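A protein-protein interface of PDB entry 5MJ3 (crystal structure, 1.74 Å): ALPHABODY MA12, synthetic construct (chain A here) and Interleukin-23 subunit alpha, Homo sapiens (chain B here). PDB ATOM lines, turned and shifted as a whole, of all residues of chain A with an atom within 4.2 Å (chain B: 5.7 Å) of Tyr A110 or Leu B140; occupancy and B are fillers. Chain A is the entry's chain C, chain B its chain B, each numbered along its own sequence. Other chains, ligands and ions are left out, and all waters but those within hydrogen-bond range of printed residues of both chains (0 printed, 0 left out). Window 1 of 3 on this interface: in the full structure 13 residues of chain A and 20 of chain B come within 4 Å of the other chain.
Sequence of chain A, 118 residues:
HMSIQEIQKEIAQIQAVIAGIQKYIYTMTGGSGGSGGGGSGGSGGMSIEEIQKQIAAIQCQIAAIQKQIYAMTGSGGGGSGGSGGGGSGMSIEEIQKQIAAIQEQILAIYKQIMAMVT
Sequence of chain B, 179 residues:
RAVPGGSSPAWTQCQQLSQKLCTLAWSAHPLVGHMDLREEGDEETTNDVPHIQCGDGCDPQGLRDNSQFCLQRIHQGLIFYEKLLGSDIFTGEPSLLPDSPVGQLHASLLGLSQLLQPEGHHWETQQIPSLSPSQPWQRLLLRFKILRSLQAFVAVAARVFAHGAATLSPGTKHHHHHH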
ATOM      1  N   ILE A 106      -0.922 -11.393  -6.798  1.00  0.00           N
ATOM      2  CA  ILE A 106      -0.630 -10.342  -5.830  1.00  0.00           C
ATOM      3  C   ILE A 106      -0.277 -10.949  -4.480  1.00  0.00           C
ATOM      4  O   ILE A 106       0.639 -10.484  -3.792  1.00  0.00           O
ATOM      5  CB  ILE A 106      -1.819  -9.364  -5.715  1.00  0.00           C
ATOM      6  CG1 ILE A 106      -1.954  -8.590  -7.018  1.00  0.00           C
ATOM      7  CG2 ILE A 106      -1.616  -8.386  -4.571  1.00  0.00           C
ATOM      8  CD1 ILE A 106      -3.239  -7.764  -7.128  1.00  0.00           C
ATOM      9  N   LEU A 107      -1.002 -11.992  -4.075  1.00  0.00           N
ATOM     10  CA  LEU A 107      -0.715 -12.630  -2.793  1.00  0.00           C
ATOM     11  C   LEU A 107       0.672 -13.259  -2.788  1.00  0.00           C
ATOM     12  O   LEU A 107       1.389 -13.201  -1.779  1.00  0.00           O
ATOM     13  CB  LEU A 107      -1.789 -13.678  -2.491  1.00  0.00           C
ATOM     14  CG  LEU A 107      -3.146 -13.087  -2.071  1.00  0.00           C
ATOM     15  CD1 LEU A 107      -4.252 -14.158  -2.149  1.00  0.00           C
ATOM     16  CD2 LEU A 107      -3.069 -12.524  -0.675  1.00  0.00           C
ATOM     17  N   ALA A 108       1.056 -13.888  -3.894  1.00  0.00           N
ATOM     18  CA  ALA A 108       2.393 -14.459  -3.995  1.00  0.00           C
ATOM     19  C   ALA A 108       3.471 -13.384  -3.889  1.00  0.00           C
ATOM     20  O   ALA A 108       4.489 -13.585  -3.212  1.00  0.00           O
ATOM     21  CB  ALA A 108       2.525 -15.231  -5.307  1.00  0.00           C
ATOM     22  N   ILE A 109       3.275 -12.247  -4.568  1.00  0.00           N
ATOM     23  CA  ILE A 109       4.225 -11.133  -4.484  1.00  0.00           C
ATOM     24  C   ILE A 109       4.280 -10.589  -3.063  1.00  0.00           C
ATOM     25  O   ILE A 109       5.357 -10.324  -2.516  1.00  0.00           O
ATOM     26  CB  ILE A 109       3.837 -10.020  -5.479  1.00  0.00           C
ATOM     27  CG1 ILE A 109       4.027 -10.498  -6.915  1.00  0.00           C
ATOM     28  CG2 ILE A 109       4.630  -8.730  -5.196  1.00  0.00           C
ATOM     29  CD1 ILE A 109       3.414  -9.580  -7.948  1.00  0.00           C
ATOM     30  N   TYR A 110       3.110 -10.340  -2.475  1.00  0.00           N
ATOM     31  CA  TYR A 110       3.039  -9.872  -1.100  1.00  0.00           C
ATOM     32  C   TYR A 110       3.809 -10.797  -0.162  1.00  0.00           C
ATOM     33  O   TYR A 110       4.594 -10.343   0.679  1.00  0.00           O
ATOM     34  CB  TYR A 110       1.568  -9.766  -0.696  1.00  0.00           C
ATOM     35  CG  TYR A 110       1.305  -9.418   0.753  1.00  0.00           C
ATOM     36  CD1 TYR A 110       1.174  -8.097   1.165  1.00  0.00           C
ATOM     37  CD2 TYR A 110       1.145 -10.415   1.697  1.00  0.00           C
ATOM     38  CE1 TYR A 110       0.906  -7.778   2.500  1.00  0.00           C
ATOM     39  CE2 TYR A 110       0.894 -10.113   3.018  1.00  0.00           C
ATOM     40  CZ  TYR A 110       0.761  -8.801   3.411  1.00  0.00           C
ATOM     41  OH  TYR A 110       0.485  -8.536   4.722  1.00  0.00           O
ATOM     42  N   LYS A 111       3.615 -12.105  -0.303  1.00  0.00           N
ATOM     43  CA  LYS A 111       4.335 -13.034   0.564  1.00  0.00           C
ATOM     44  C   LYS A 111       5.839 -12.946   0.340  1.00  0.00           C
ATOM     45  O   LYS A 111       6.614 -13.014   1.297  1.00  0.00           O
ATOM     46  CB  LYS A 111       3.830 -14.460   0.356  1.00  0.00           C
ATOM     47  CG  LYS A 111       2.466 -14.690   1.005  1.00  0.00           C
ATOM     48  CD  LYS A 111       2.073 -16.161   1.071  1.00  0.00           C
ATOM     49  CE  LYS A 111       1.741 -16.747  -0.281  1.00  0.00           C
ATOM     50  NZ  LYS A 111       1.131 -18.109  -0.141  1.00  0.00           N
ATOM     51  N   GLN A 112       6.277 -12.798  -0.913  1.00  0.00           N
ATOM     52  CA  GLN A 112       7.710 -12.636  -1.168  1.00  0.00           C
ATOM     53  C   GLN A 112       8.260 -11.393  -0.480  1.00  0.00           C
ATOM     54  O   GLN A 112       9.327 -11.431   0.141  1.00  0.00           O
ATOM     55  CB  GLN A 112       7.983 -12.559  -2.672  1.00  0.00           C
ATOM     56  CG  GLN A 112       7.930 -13.892  -3.390  1.00  0.00           C
ATOM     57  CD  GLN A 112       8.498 -13.826  -4.798  1.00  0.00           C
ATOM     58  OE1 GLN A 112       8.579 -12.756  -5.402  1.00  0.00           O
ATOM     59  NE2 GLN A 112       8.897 -14.976  -5.325  1.00  0.00           N
ATOM     60  N   ILE A 113       7.559 -10.266  -0.613  1.00  0.00           N
ATOM     61  CA  ILE A 113       8.019  -9.014  -0.009  1.00  0.00           C
ATOM     62  C   ILE A 113       8.035  -9.118   1.509  1.00  0.00           C
ATOM     63  O   ILE A 113       8.977  -8.669   2.170  1.00  0.00           O
ATOM     64  CB  ILE A 113       7.131  -7.840  -0.471  1.00  0.00           C
ATOM     65  CG1 ILE A 113       7.269  -7.627  -1.981  1.00  0.00           C
ATOM     66  CG2 ILE A 113       7.488  -6.574   0.283  1.00  0.00           C
ATOM     67  CD1 ILE A 113       8.637  -7.163  -2.419  1.00  0.00           C
ATOM     68  N   MET A 114       6.969  -9.666   2.093  1.00  0.00           N
ATOM     69  CA  MET A 114       6.946  -9.790   3.548  1.00  0.00           C
ATOM     70  C   MET A 114       8.089 -10.671   4.035  1.00  0.00           C
ATOM     71  O   MET A 114       8.677 -10.418   5.097  1.00  0.00           O
ATOM     72  CB  MET A 114       5.601 -10.349   4.017  1.00  0.00           C
ATOM     73  CG  MET A 114       4.438  -9.360   3.962  1.00  0.00           C
ATOM     74  SD  MET A 114       4.749  -7.808   4.850  1.00  0.00           S
ATOM     75  CE  MET A 114       5.058  -6.736   3.461  1.00  0.00           C
ATOM     76  N   HIS B  29       4.030  -1.849   6.862  1.00  0.00           N
ATOM     77  CA  HIS B  29       3.166  -2.619   5.980  1.00  0.00           C
ATOM     78  C   HIS B  29       2.778  -1.716   4.826  1.00  0.00           C
ATOM     79  O   HIS B  29       2.695  -0.491   5.003  1.00  0.00           O
ATOM     80  CB  HIS B  29       1.914  -3.102   6.741  1.00  0.00           C
ATOM     81  CG  HIS B  29       1.059  -4.082   5.998  1.00  0.00           C
ATOM     82  ND1 HIS B  29       0.116  -3.695   5.069  1.00  0.00           N
ATOM     83  CD2 HIS B  29       0.969  -5.434   6.081  1.00  0.00           C
ATOM     84  CE1 HIS B  29      -0.487  -4.766   4.585  1.00  0.00           C
ATOM     85  NE2 HIS B  29      -0.005  -5.829   5.198  1.00  0.00           N
ATOM     86  N   PRO B  30       2.538  -2.271   3.639  1.00  0.00           N
ATOM     87  CA  PRO B  30       2.017  -1.442   2.546  1.00  0.00           C
ATOM     88  C   PRO B  30       0.747  -0.701   2.947  1.00  0.00           C
ATOM     89  O   PRO B  30      -0.005  -1.131   3.826  1.00  0.00           O
ATOM     90  CB  PRO B  30       1.740  -2.456   1.431  1.00  0.00           C
ATOM     91  CG  PRO B  30       2.634  -3.568   1.699  1.00  0.00           C
ATOM     92  CD  PRO B  30       2.792  -3.649   3.192  1.00  0.00           C
ATOM     93  N   ILE B  89      -6.185 -12.574  11.769  1.00  0.00           N
ATOM     94  CA  ILE B  89      -6.188 -11.602  10.680  1.00  0.00           C
ATOM     95  C   ILE B  89      -4.771 -11.410  10.159  1.00  0.00           C
ATOM     96  O   ILE B  89      -4.550 -11.301   8.946  1.00  0.00           O
ATOM     97  CB  ILE B  89      -6.798 -10.272  11.151  1.00  0.00           C
ATOM     98  CG1 ILE B  89      -8.256 -10.480  11.568  1.00  0.00           C
ATOM     99  CG2 ILE B  89      -6.683  -9.201  10.047  1.00  0.00           C
ATOM    100  CD1 ILE B  89      -8.838  -9.309  12.370  1.00  0.00           C
ATOM    101  N   PRO B  94      -2.303 -14.824   4.108  1.00  0.00           N
ATOM    102  CA  PRO B  94      -0.842 -14.911   3.996  1.00  0.00           C
ATOM    103  C   PRO B  94      -0.155 -14.487   5.299  1.00  0.00           C
ATOM    104  O   PRO B  94      -0.257 -13.335   5.702  1.00  0.00           O
ATOM    105  CB  PRO B  94      -0.528 -13.943   2.857  1.00  0.00           C
ATOM    106  CG  PRO B  94      -1.589 -12.892   2.971  1.00  0.00           C
ATOM    107  CD  PRO B  94      -2.820 -13.604   3.456  1.00  0.00           C
ATOM    108  N   LEU B  96       1.987 -13.396   8.522  1.00  0.00           N
ATOM    109  CA  LEU B  96       3.074 -12.548   8.980  1.00  0.00           C
ATOM    110  C   LEU B  96       3.701 -13.160  10.226  1.00  0.00           C
ATOM    111  O   LEU B  96       2.995 -13.638  11.121  1.00  0.00           O
ATOM    112  CB  LEU B  96       2.571 -11.134   9.284  1.00  0.00           C
ATOM    113  CG  LEU B  96       1.842 -10.473   8.113  1.00  0.00           C
ATOM    114  CD1 LEU B  96       1.377  -9.073   8.472  1.00  0.00           C
ATOM    115  CD2 LEU B  96       2.741 -10.455   6.880  1.00  0.00           C
ATOM    116  N   GLN B 135     -10.910 -16.116   3.852  1.00  0.00           N
ATOM    117  CA  GLN B 135     -10.218 -16.104   2.562  1.00  0.00           C
ATOM    118  C   GLN B 135      -8.949 -15.254   2.660  1.00  0.00           C
ATOM    119  O   GLN B 135      -8.998 -14.161   3.220  1.00  0.00           O
ATOM    120  CB  GLN B 135     -11.116 -15.542   1.467  1.00  0.00           C
ATOM    121  CG  GLN B 135     -12.093 -16.536   0.878  1.00  0.00           C
ATOM    122  CD  GLN B 135     -11.394 -17.625   0.078  1.00  0.00           C
ATOM    123  OE1 GLN B 135     -10.761 -17.358  -0.947  1.00  0.00           O
ATOM    124  NE2 GLN B 135     -11.489 -18.854   0.555  1.00  0.00           N
ATOM    125  N   PRO B 136      -7.809 -15.714   2.129  1.00  0.00           N
ATOM    126  CA  PRO B 136      -6.574 -14.905   2.201  1.00  0.00           C
ATOM    127  C   PRO B 136      -6.697 -13.494   1.633  1.00  0.00           C
ATOM    128  O   PRO B 136      -6.146 -12.558   2.218  1.00  0.00           O
ATOM    129  CB  PRO B 136      -5.570 -15.747   1.404  1.00  0.00           C
ATOM    130  CG  PRO B 136      -6.026 -17.177   1.622  1.00  0.00           C
ATOM    131  CD  PRO B 136      -7.547 -17.086   1.650  1.00  0.00           C
ATOM    132  N   TRP B 137      -7.368 -13.310   0.492  1.00  0.00           N
ATOM    133  CA  TRP B 137      -7.516 -11.963  -0.051  1.00  0.00           C
ATOM    134  C   TRP B 137      -8.265 -11.059   0.922  1.00  0.00           C
ATOM    135  O   TRP B 137      -7.906  -9.886   1.096  1.00  0.00           O
ATOM    136  CB  TRP B 137      -8.232 -12.006  -1.409  1.00  0.00           C
ATOM    137  CG  TRP B 137      -8.342 -10.623  -2.052  1.00  0.00           C
ATOM    138  CD1 TRP B 137      -9.449  -9.830  -2.114  1.00  0.00           C
ATOM    139  CD2 TRP B 137      -7.287  -9.885  -2.685  1.00  0.00           C
ATOM    140  NE1 TRP B 137      -9.153  -8.640  -2.744  1.00  0.00           N
ATOM    141  CE2 TRP B 137      -7.832  -8.654  -3.115  1.00  0.00           C
ATOM    142  CE3 TRP B 137      -5.938 -10.157  -2.941  1.00  0.00           C
ATOM    143  CZ2 TRP B 137      -7.069  -7.690  -3.769  1.00  0.00           C
ATOM    144  CZ3 TRP B 137      -5.185  -9.204  -3.599  1.00  0.00           C
ATOM    145  CH2 TRP B 137      -5.749  -7.989  -4.005  1.00  0.00           C
ATOM    146  N   GLN B 138      -9.312 -11.582   1.565  1.00  0.00           N
ATOM    147  CA  GLN B 138     -10.066 -10.763   2.507  1.00  0.00           C
ATOM    148  C   GLN B 138      -9.259 -10.475   3.766  1.00  0.00           C
ATOM    149  O   GLN B 138      -9.382  -9.384   4.329  1.00  0.00           O
ATOM    150  CB  GLN B 138     -11.395 -11.427   2.866  1.00  0.00           C
ATOM    151  CG  GLN B 138     -12.345 -11.594   1.683  1.00  0.00           C
ATOM    152  CD  GLN B 138     -12.767 -10.268   1.036  1.00  0.00           C
ATOM    153  OE1 GLN B 138     -12.960  -9.258   1.711  1.00  0.00           O
ATOM    154  NE2 GLN B 138     -12.908 -10.282  -0.281  1.00  0.00           N
ATOM    155  N   ARG B 139      -8.408 -11.408   4.208  1.00  0.00           N
ATOM    156  CA  ARG B 139      -7.506 -11.095   5.313  1.00  0.00           C
ATOM    157  C   ARG B 139      -6.629  -9.910   4.955  1.00  0.00           C
ATOM    158  O   ARG B 139      -6.456  -8.981   5.751  1.00  0.00           O
ATOM    159  CB  ARG B 139      -6.615 -12.290   5.674  1.00  0.00           C
ATOM    160  CG  ARG B 139      -7.232 -13.262   6.634  1.00  0.00           C
ATOM    161  CD  ARG B 139      -6.188 -14.176   7.284  1.00  0.00           C
ATOM    162  NE  ARG B 139      -6.857 -15.321   7.872  1.00  0.00           N
ATOM    163  CZ  ARG B 139      -7.088 -16.460   7.233  1.00  0.00           C
ATOM    164  NH1 ARG B 139      -6.680 -16.621   5.977  1.00  0.00           N
ATOM    165  NH2 ARG B 139      -7.718 -17.449   7.859  1.00  0.00           N
ATOM    166  N   LEU B 140      -6.046  -9.945   3.755  1.00  0.00           N
ATOM    167  CA  LEU B 140      -5.159  -8.875   3.317  1.00  0.00           C
ATOM    168  C   LEU B 140      -5.878  -7.535   3.294  1.00  0.00           C
ATOM    169  O   LEU B 140      -5.368  -6.537   3.820  1.00  0.00           O
ATOM    170  CB  LEU B 140      -4.583  -9.223   1.945  1.00  0.00           C
ATOM    171  CG  LEU B 140      -3.687  -8.174   1.284  1.00  0.00           C
ATOM    172  CD1 LEU B 140      -2.502  -7.842   2.174  1.00  0.00           C
ATOM    173  CD2 LEU B 140      -3.205  -8.633  -0.079  1.00  0.00           C
ATOM    174  N   LEU B 141      -7.087  -7.489   2.727  1.00  0.00           N
ATOM    175  CA  LEU B 141      -7.804  -6.214   2.707  1.00  0.00           C
ATOM    176  C   LEU B 141      -8.032  -5.698   4.119  1.00  0.00           C
ATOM    177  O   LEU B 141      -7.873  -4.497   4.388  1.00  0.00           O
ATOM    178  CB  LEU B 141      -9.147  -6.356   1.984  1.00  0.00           C
ATOM    179  CG  LEU B 141      -9.098  -6.692   0.494  1.00  0.00           C
ATOM    180  CD1 LEU B 141     -10.526  -6.812  -0.040  1.00  0.00           C
ATOM    181  CD2 LEU B 141      -8.335  -5.648  -0.292  1.00  0.00           C
ATOM    182  N   LEU B 142      -8.403  -6.593   5.040  1.00  0.00           N
ATOM    183  CA  LEU B 142      -8.698  -6.160   6.397  1.00  0.00           C
ATOM    184  C   LEU B 142      -7.451  -5.629   7.083  1.00  0.00           C
ATOM    185  O   LEU B 142      -7.559  -4.741   7.934  1.00  0.00           O
ATOM    186  CB  LEU B 142      -9.328  -7.307   7.201  1.00  0.00           C
ATOM    187  CG  LEU B 142      -9.827  -6.985   8.623  1.00  0.00           C
ATOM    188  CD1 LEU B 142     -10.844  -5.843   8.634  1.00  0.00           C
ATOM    189  CD2 LEU B 142     -10.438  -8.235   9.254  1.00  0.00           C
ATOM    190  N   ARG B 143      -6.268  -6.143   6.725  1.00  0.00           N
ATOM    191  CA  ARG B 143      -5.028  -5.625   7.302  1.00  0.00           C
ATOM    192  C   ARG B 143      -4.831  -4.163   6.972  1.00  0.00           C
ATOM    193  O   ARG B 143      -4.435  -3.371   7.838  1.00  0.00           O
ATOM    194  CB  ARG B 143      -3.826  -6.408   6.801  1.00  0.00           C
ATOM    195  CG  ARG B 143      -3.773  -7.766   7.364  1.00  0.00           C
ATOM    196  CD  ARG B 143      -2.609  -8.514   6.835  1.00  0.00           C
ATOM    197  NE  ARG B 143      -2.823  -9.916   7.176  1.00  0.00           N
ATOM    198  CZ  ARG B 143      -2.095 -10.930   6.744  1.00  0.00           C
ATOM    199  NH1 ARG B 143      -1.039 -10.736   5.959  1.00  0.00           N
ATOM    200  NH2 ARG B 143      -2.439 -12.150   7.120  1.00  0.00           N
ATOM    201  N   PHE B 144      -5.079  -3.784   5.719  1.00  0.00           N
ATOM    202  CA  PHE B 144      -4.981  -2.375   5.360  1.00  0.00           C
ATOM    203  C   PHE B 144      -5.926  -1.537   6.202  1.00  0.00           C
ATOM    204  O   PHE B 144      -5.557  -0.454   6.669  1.00  0.00           O
ATOM    205  CB  PHE B 144      -5.298  -2.151   3.879  1.00  0.00           C
ATOM    206  CG  PHE B 144      -4.254  -2.650   2.945  1.00  0.00           C
ATOM    207  CD1 PHE B 144      -3.081  -1.941   2.763  1.00  0.00           C
ATOM    208  CD2 PHE B 144      -4.462  -3.804   2.205  1.00  0.00           C
ATOM    209  CE1 PHE B 144      -2.118  -2.378   1.878  1.00  0.00           C
ATOM    210  CE2 PHE B 144      -3.484  -4.268   1.328  1.00  0.00           C
ATOM    211  CZ  PHE B 144      -2.315  -3.559   1.164  1.00  0.00           C
ATOM    212  N   LYS B 145      -7.158  -2.014   6.384  1.00  0.00           N
ATOM    213  CA  LYS B 145      -8.158  -1.244   7.117  1.00  0.00           C
ATOM    214  C   LYS B 145      -7.811  -1.133   8.589  1.00  0.00           C
ATOM    215  O   LYS B 145      -8.001  -0.077   9.202  1.00  0.00           O
ATOM    216  CB  LYS B 145      -9.537  -1.883   6.947  1.00  0.00           C
ATOM    217  CG  LYS B 145      -9.994  -1.970   5.501  1.00  0.00           C
ATOM    218  CD  LYS B 145     -11.346  -2.685   5.418  1.00  0.00           C
ATOM    219  CE  LYS B 145     -11.821  -2.836   3.991  1.00  0.00           C
ATOM    220  NZ  LYS B 145     -13.194  -3.447   3.916  1.00  0.00           N
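Among the printed residues, pairs that only touch across the chains: Tyr A110 with Leu B140 (3.4 Å), Met A114 with Leu B96 (3.5 Å), Lys A111 with Pro B94 (3.6 Å), Tyr A110 with Leu B96 (3.7 Å), Tyr A110 with Pro B94 (3.7 Å), Ile A106 with Trp B137 (3.8 Å), Met A114 with Pro B30 (3.8 Å), Leu A107 with Leu B140 (3.9 Å) and Leu A107 with Pro B94 (3.95 Å).
Of the printed residues of chain B, Leu A107 touches Pro B94 and Leu B140. Ile A113 touches none of the printed residues of chain B. Of the printed residues of chain B, Met A114 touches Pro B30 and Leu B96. Printed residues of chain A within 4 Å of Pro B94: Leu A107, Tyr A110 and Lys A111. Of the printed residues of chain A, Leu B140 touches Leu A107 (3.9 Å) and Tyr A110 (3.4 Å). The nearest residue of chain B that does not touch Tyr A110 is Pro B30 (4.6 Å). The nearest printed residue of chain A that does not touch Leu B140 is Ile A106 (4.8 Å). The nearest printed residue of chain A that does not touch His B29 is Met A114 (4.6 Å).
Hydrophobic or aromatic side chains of chain A that line the printed part of chain B: Ile A106, Leu A107, Tyr A110 and Met A114. Hydrophobic or aromatic side chains of chain B within 4 Å of the printed part of chain A: His B29, Pro B30, Pro B94, Leu B96, Trp B137 and Leu B140. Among the printed residues, 11 pairs touch across the chains.
A ring nitrogen (NE2) of His B29 lies within hydrogen-bond range of the side-chain hydroxyl (OH) of Tyr A110 (2.8 Å). OH of Tyr A110 lies within hydrogen-bond range of NH1 of Arg B143, 2.9 Å away.
The guanidinium group of Arg B143 is in hydrogen-bond range of the backbone carbonyl oxygen of Ile B89, 2.8 Å away. NH1 of Arg B143 sits at hydrogen-bond distance from O of Pro B94 (2.7 Å).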
